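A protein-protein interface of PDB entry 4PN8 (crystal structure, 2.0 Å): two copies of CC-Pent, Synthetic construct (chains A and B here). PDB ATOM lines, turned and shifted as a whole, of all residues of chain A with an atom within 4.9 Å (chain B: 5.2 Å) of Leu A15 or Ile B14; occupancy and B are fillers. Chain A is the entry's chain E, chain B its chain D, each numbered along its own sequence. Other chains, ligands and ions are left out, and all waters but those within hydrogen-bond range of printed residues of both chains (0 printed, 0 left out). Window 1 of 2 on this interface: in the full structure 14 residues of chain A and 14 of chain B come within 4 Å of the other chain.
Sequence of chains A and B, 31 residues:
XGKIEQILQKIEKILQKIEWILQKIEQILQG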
ATOM      1  N   ILE A  11      30.101  29.091   7.804  1.00  0.00           N
ATOM      2  CA  ILE A  11      29.115  29.834   8.591  1.00  0.00           C
ATOM      3  C   ILE A  11      28.504  28.926   9.641  1.00  0.00           C
ATOM      4  O   ILE A  11      28.356  29.307  10.801  1.00  0.00           O
ATOM      5  CB  ILE A  11      28.022  30.438   7.672  1.00  0.00           C
ATOM      6  CG1 ILE A  11      28.589  31.666   6.948  1.00  0.00           C
ATOM      7  CG2 ILE A  11      26.778  30.816   8.470  1.00  0.00           C
ATOM      8  CD1 ILE A  11      27.779  32.135   5.776  1.00  0.00           C
ATOM      9  N   GLU A  12      28.156  27.711   9.241  1.00  0.00           N
ATOM     10  CA  GLU A  12      27.662  26.731  10.190  1.00  0.00           C
ATOM     11  C   GLU A  12      28.664  26.499  11.332  1.00  0.00           C
ATOM     12  O   GLU A  12      28.286  26.465  12.501  1.00  0.00           O
ATOM     13  CB  GLU A  12      27.362  25.403   9.490  1.00  0.00           C
ATOM     14  CG  GLU A  12      26.850  24.343  10.436  1.00  0.00           C
ATOM     15  CD  GLU A  12      26.783  22.968   9.792  1.00  0.00           C
ATOM     16  OE1 GLU A  12      27.088  22.845   8.588  1.00  0.00           O
ATOM     17  OE2 GLU A  12      26.415  22.011  10.494  1.00  0.00           O
ATOM     18  N   LYS A  13      29.940  26.350  10.998  1.00  0.00           N
ATOM     19  CA  LYS A  13      30.961  26.117  12.021  1.00  0.00           C
ATOM     20  C   LYS A  13      31.119  27.297  12.972  1.00  0.00           C
ATOM     21  O   LYS A  13      31.260  27.110  14.184  1.00  0.00           O
ATOM     22  CB  LYS A  13      32.306  25.791  11.372  1.00  0.00           C
ATOM     23  CG  LYS A  13      32.352  24.418  10.727  1.00  0.00           C
ATOM     24  CD  LYS A  13      33.791  24.016  10.404  1.00  0.00           C
ATOM     25  CE  LYS A  13      33.829  22.591   9.897  1.00  0.00           C
ATOM     26  NZ  LYS A  13      32.692  22.347   8.956  1.00  0.00           N
ATOM     27  N   ILE A  14      31.109  28.512  12.434  1.00  0.00           N
ATOM     28  CA  ILE A  14      31.230  29.680  13.286  1.00  0.00           C
ATOM     29  C   ILE A  14      30.015  29.777  14.212  1.00  0.00           C
ATOM     30  O   ILE A  14      30.150  30.130  15.378  1.00  0.00           O
ATOM     31  CB  ILE A  14      31.381  30.985  12.483  1.00  0.00           C
ATOM     32  CG1 ILE A  14      32.592  30.910  11.564  1.00  0.00           C
ATOM     33  CG2 ILE A  14      31.580  32.172  13.419  1.00  0.00           C
ATOM     34  CD1 ILE A  14      32.589  31.975  10.474  1.00  0.00           C
ATOM     35  N   LEU A  15      28.830  29.466  13.695  1.00  0.00           N
ATOM     36  CA  LEU A  15      27.627  29.528  14.517  1.00  0.00           C
ATOM     37  C   LEU A  15      27.692  28.488  15.622  1.00  0.00           C
ATOM     38  O   LEU A  15      27.274  28.753  16.737  1.00  0.00           O
ATOM     39  CB  LEU A  15      26.372  29.361  13.668  1.00  0.00           C
ATOM     40  CG  LEU A  15      26.087  30.632  12.851  1.00  0.00           C
ATOM     41  CD1 LEU A  15      25.016  30.343  11.821  1.00  0.00           C
ATOM     42  CD2 LEU A  15      25.627  31.743  13.770  1.00  0.00           C
ATOM     43  N   GLN A  16      28.222  27.301  15.334  1.00  0.00           N
ATOM     44  CA  GLN A  16      28.381  26.311  16.395  1.00  0.00           C
ATOM     45  C   GLN A  16      29.321  26.827  17.476  1.00  0.00           C
ATOM     46  O   GLN A  16      29.061  26.622  18.655  1.00  0.00           O
ATOM     47  CB  GLN A  16      28.879  24.958  15.879  1.00  0.00           C
ATOM     48  CG  GLN A  16      28.944  23.910  16.986  1.00  0.00           C
ATOM     49  CD  GLN A  16      27.639  23.817  17.768  1.00  0.00           C
ATOM     50  OE1 GLN A  16      26.623  23.382  17.225  1.00  0.00           O
ATOM     51  NE2 GLN A  16      27.657  24.237  19.045  1.00  0.00           N
ATOM     52  N   LYS A  17      30.400  27.508  17.085  1.00  0.00           N
ATOM     53  CA  LYS A  17      31.309  28.071  18.086  1.00  0.00           C
ATOM     54  C   LYS A  17      30.603  29.121  18.948  1.00  0.00           C
ATOM     55  O   LYS A  17      30.785  29.159  20.164  1.00  0.00           O
ATOM     56  CB  LYS A  17      32.557  28.683  17.443  1.00  0.00           C
ATOM     57  CG  LYS A  17      33.612  27.660  17.059  1.00  0.00           C
ATOM     58  CD  LYS A  17      34.727  28.321  16.255  1.00  0.00           C
ATOM     59  CE  LYS A  17      35.703  27.287  15.706  1.00  0.00           C
ATOM     60  NZ  LYS A  17      36.824  27.962  14.996  1.00  0.00           N
ATOM     61  N   ILE A  18      29.799  29.965  18.303  1.00  0.00           N
ATOM     62  CA  ILE A  18      29.056  31.014  18.990  1.00  0.00           C
ATOM     63  C   ILE A  18      28.071  30.423  19.986  1.00  0.00           C
ATOM     64  O   ILE A  18      27.968  30.892  21.114  1.00  0.00           O
ATOM     65  CB  ILE A  18      28.290  31.880  17.967  1.00  0.00           C
ATOM     66  CG1 ILE A  18      29.274  32.832  17.276  1.00  0.00           C
ATOM     67  CG2 ILE A  18      27.154  32.660  18.650  1.00  0.00           C
ATOM     68  CD1 ILE A  18      28.739  33.503  16.023  1.00  0.00           C
ATOM     69  N   GLU A  19      27.331  29.401  19.566  1.00  0.00           N
ATOM     70  CA  GLU A  19      26.377  28.764  20.465  1.00  0.00           C
ATOM     71  C   GLU A  19      27.079  28.169  21.676  1.00  0.00           C
ATOM     72  O   GLU A  19      26.565  28.226  22.792  1.00  0.00           O
ATOM     73  CB  GLU A  19      25.592  27.658  19.766  1.00  0.00           C
ATOM     74  CG  GLU A  19      24.588  26.975  20.706  1.00  0.00           C
ATOM     75  CD  GLU A  19      24.241  25.555  20.291  1.00  0.00           C
ATOM     76  OE1 GLU A  19      24.443  25.196  19.105  1.00  0.00           O
ATOM     77  OE2 GLU A  19      23.742  24.801  21.155  1.00  0.00           O
ATOM     78  N   LYS B  10      20.529  23.183   8.989  1.00  0.00           N
ATOM     79  CA  LYS B  10      21.384  23.081  10.172  1.00  0.00           C
ATOM     80  C   LYS B  10      21.715  24.448  10.778  1.00  0.00           C
ATOM     81  O   LYS B  10      21.712  24.618  12.003  1.00  0.00           O
ATOM     82  CB  LYS B  10      22.645  22.292   9.854  1.00  0.00           C
ATOM     83  CG  LYS B  10      22.341  20.816   9.631  1.00  0.00           C
ATOM     84  CD  LYS B  10      23.549  20.075   9.060  1.00  0.00           C
ATOM     85  CE  LYS B  10      23.190  18.638   8.661  1.00  0.00           C
ATOM     86  NZ  LYS B  10      24.431  17.845   8.352  1.00  0.00           N
ATOM     87  N   ILE B  11      21.975  25.429   9.922  1.00  0.00           N
ATOM     88  CA  ILE B  11      22.204  26.804  10.373  1.00  0.00           C
ATOM     89  C   ILE B  11      20.983  27.361  11.118  1.00  0.00           C
ATOM     90  O   ILE B  11      21.112  28.004  12.165  1.00  0.00           O
ATOM     91  CB  ILE B  11      22.572  27.693   9.168  1.00  0.00           C
ATOM     92  CG1 ILE B  11      24.047  27.459   8.790  1.00  0.00           C
ATOM     93  CG2 ILE B  11      22.326  29.150   9.470  1.00  0.00           C
ATOM     94  CD1 ILE B  11      24.416  27.940   7.370  1.00  0.00           C
ATOM     95  N   GLU B  12      19.797  27.106  10.578  1.00  0.00           N
ATOM     96  CA  GLU B  12      18.545  27.525  11.205  1.00  0.00           C
ATOM     97  C   GLU B  12      18.394  26.976  12.630  1.00  0.00           C
ATOM     98  O   GLU B  12      17.967  27.686  13.547  1.00  0.00           O
ATOM     99  CB  GLU B  12      17.351  27.076  10.351  1.00  0.00           C
ATOM    100  CG  GLU B  12      16.000  27.521  10.916  1.00  0.00           C
ATOM    101  CD  GLU B  12      14.805  26.784  10.284  1.00  0.00           C
ATOM    102  OE1 GLU B  12      13.673  26.948  10.785  1.00  0.00           O
ATOM    103  OE2 GLU B  12      14.988  26.046   9.289  1.00  0.00           O
ATOM    104  N   LYS B  13      18.747  25.712  12.822  1.00  0.00           N
ATOM    105  CA  LYS B  13      18.577  25.083  14.117  1.00  0.00           C
ATOM    106  C   LYS B  13      19.592  25.597  15.127  1.00  0.00           C
ATOM    107  O   LYS B  13      19.280  25.729  16.308  1.00  0.00           O
ATOM    108  CB  LYS B  13      18.658  23.569  13.972  1.00  0.00           C
ATOM    109  CG  LYS B  13      17.467  23.010  13.201  1.00  0.00           C
ATOM    110  CD  LYS B  13      17.729  21.604  12.671  1.00  0.00           C
ATOM    111  CE  LYS B  13      16.532  21.097  11.886  1.00  0.00           C
ATOM    112  NZ  LYS B  13      15.300  21.124  12.720  1.00  0.00           N
ATOM    113  N   ILE B  14      20.804  25.892  14.667  1.00  0.00           N
ATOM    114  CA  ILE B  14      21.813  26.447  15.560  1.00  0.00           C
ATOM    115  C   ILE B  14      21.381  27.838  16.006  1.00  0.00           C
ATOM    116  O   ILE B  14      21.501  28.186  17.189  1.00  0.00           O
ATOM    117  CB  ILE B  14      23.194  26.542  14.888  1.00  0.00           C
ATOM    118  CG1 ILE B  14      23.668  25.161  14.457  1.00  0.00           C
ATOM    119  CG2 ILE B  14      24.210  27.135  15.852  1.00  0.00           C
ATOM    120  CD1 ILE B  14      24.891  25.208  13.541  1.00  0.00           C
ATOM    121  N   LEU B  15      20.883  28.633  15.058  1.00  0.00           N
ATOM    122  CA  LEU B  15      20.373  29.968  15.387  1.00  0.00           C
ATOM    123  C   LEU B  15      19.201  29.897  16.349  1.00  0.00           C
ATOM    124  O   LEU B  15      19.063  30.745  17.231  1.00  0.00           O
ATOM    125  CB  LEU B  15      19.960  30.726  14.124  1.00  0.00           C
ATOM    126  CG  LEU B  15      21.145  31.211  13.279  1.00  0.00           C
ATOM    127  CD1 LEU B  15      20.657  31.755  11.932  1.00  0.00           C
ATOM    128  CD2 LEU B  15      21.930  32.296  14.022  1.00  0.00           C
ATOM    129  N   GLN B  16      18.339  28.904  16.198  1.00  0.00           N
ATOM    130  CA  GLN B  16      17.225  28.813  17.149  1.00  0.00           C
ATOM    131  C   GLN B  16      17.756  28.495  18.545  1.00  0.00           C
ATOM    132  O   GLN B  16      17.284  29.049  19.546  1.00  0.00           O
ATOM    133  CB  GLN B  16      16.188  27.778  16.720  1.00  0.00           C
ATOM    134  CG  GLN B  16      15.059  27.665  17.737  1.00  0.00           C
ATOM    135  CD  GLN B  16      14.380  29.011  18.018  1.00  0.00           C
ATOM    136  OE1 GLN B  16      14.548  29.609  19.093  1.00  0.00           O
ATOM    137  NE2 GLN B  16      13.603  29.480  17.059  1.00  0.00           N
ATOM    138  N   LYS B  17      18.762  27.630  18.613  1.00  0.00           N
ATOM    139  CA  LYS B  17      19.396  27.303  19.885  1.00  0.00           C
ATOM    140  C   LYS B  17      20.051  28.523  20.513  1.00  0.00           C
ATOM    141  O   LYS B  17      19.967  28.739  21.734  1.00  0.00           O
ATOM    142  CB  LYS B  17      20.440  26.202  19.686  1.00  0.00           C
ATOM    143  CG  LYS B  17      19.824  24.820  19.456  1.00  0.00           C
ATOM    144  CD  LYS B  17      20.907  23.742  19.300  1.00  0.00           C
ATOM    145  CE  LYS B  17      20.255  22.371  19.084  1.00  0.00           C
ATOM    146  NZ  LYS B  17      21.252  21.303  18.804  1.00  0.00           N
ATOM    147  N   ILE B  18      20.709  29.324  19.683  1.00  0.00           N
ATOM    148  CA  ILE B  18      21.285  30.578  20.160  1.00  0.00           C
ATOM    149  C   ILE B  18      20.210  31.513  20.721  1.00  0.00           C
ATOM    150  O   ILE B  18      20.396  32.107  21.782  1.00  0.00           O
ATOM    151  CB  ILE B  18      22.057  31.294  19.026  1.00  0.00           C
ATOM    152  CG1 ILE B  18      23.369  30.549  18.741  1.00  0.00           C
ATOM    153  CG2 ILE B  18      22.327  32.764  19.391  1.00  0.00           C
ATOM    154  CD1 ILE B  18      23.912  30.769  17.327  1.00  0.00           C
ATOM    155  N   GLU B  19      19.085  31.643  20.016  1.00  0.00           N
ATOM    156  CA  GLU B  19      18.013  32.542  20.459  1.00  0.00           C
ATOM    157  C   GLU B  19      17.457  32.086  21.802  1.00  0.00           C
ATOM    158  O   GLU B  19      17.150  32.909  22.668  1.00  0.00           O
ATOM    159  CB  GLU B  19      16.891  32.600  19.427  1.00  0.00           C
ATOM    160  CG  GLU B  19      15.749  33.553  19.776  1.00  0.00           C
ATOM    161  CD  GLU B  19      14.411  33.046  19.266  1.00  0.00           C
ATOM    162  OE1 GLU B  19      14.197  33.016  18.028  1.00  0.00           O
ATOM    163  OE2 GLU B  19      13.574  32.656  20.101  1.00  0.00           O
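CG2 of Ile A11 touches CD1 of Ile B11, at 3.9 Å.
Glu A12 touches Lys B10.
Ile B11 touches Glu A12 (CG1 to CA, 3.9 Å).
Leu A15 touches Ile B11 (CD1 to CG2, 3.8 Å).
Leu A15 touches Ile B14 (O to CG2, 3.6 Å).
Leu A15 touches Leu B15.
Leu A15 touches Ile B18.
CG2 of Ile A18 touches CD1 of Ile B18, 3.98 Å away.
Glu A19 touches Lys B17 (OE2 to CD, 3.5 Å).
Glu A19 touches Ile B18.
NE2 of Gln A16 lies within hydrogen-bond range of OE1 of Glu A19, 3.4 Å away.
Glu A12 touches Ile B11, but with the chains exchanged Ile A11 does not touch Glu B12 (8.2 Å).
Leu A15 touches Ile B11, but with the chains exchanged Ile A11 does not touch Leu B15 (7.1 Å).
Ile B18 touches its own counterpart, Ile A18.
Glu A19 touches Ile B14, but with the chains exchanged Ile A14 does not touch Glu B19 (12.1 Å).
Positions printed for both chains: 11, 12, 13, 14, 15, 16, 17, 18 and 19.
Of the 12 pairs that touch across the chains among the printed residues, 3 have their exchanged pair printed and touching as well.
Of the 10 printed residues of chain B, 6 touch a printed residue of chain A.
Hydrophobic or aromatic side chains of chain B within 4 Å of the printed part of chain A: Ile B11, Ile B14, Leu B15 and Ile B18.
Among the printed residues, 12 pairs touch across the chains.
Among the printed residues, no Asp or Glu carboxylate lies within 4 Å of a Lys or Arg side-chain nitrogen of the other chain.
Of the printed residues of chain A, Ile B14 touches Glu A12 (3.8 Å), Leu A15 (3.6 Å) and Glu A19 (3.8 Å).
Printed residues of chain A within 4 Å of Ile B18: Leu A15, Ile A18 and Glu A19.
Of the printed residues of chain B, Glu A19 touches Ile B14 (3.8 Å), Lys B17 (3.5 Å) and Ile B18 (3.8 Å).
Printed residues of chain A within 4 Å of Ile B11: Ile A11, Glu A12 and Leu A15.
Printed residues of chain A within 4 Å of Lys B10: Glu A12.
The nearest printed residue of chain B that does not touch Leu A15 is Glu B12 (6.3 Å).
The nearest printed residue of chain A that does not touch Ile B14 is Gln A16 (4.05 Å).
The nearest printed residue of chain B that does not touch Ile A11 is Ile B14 (6.0 Å).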
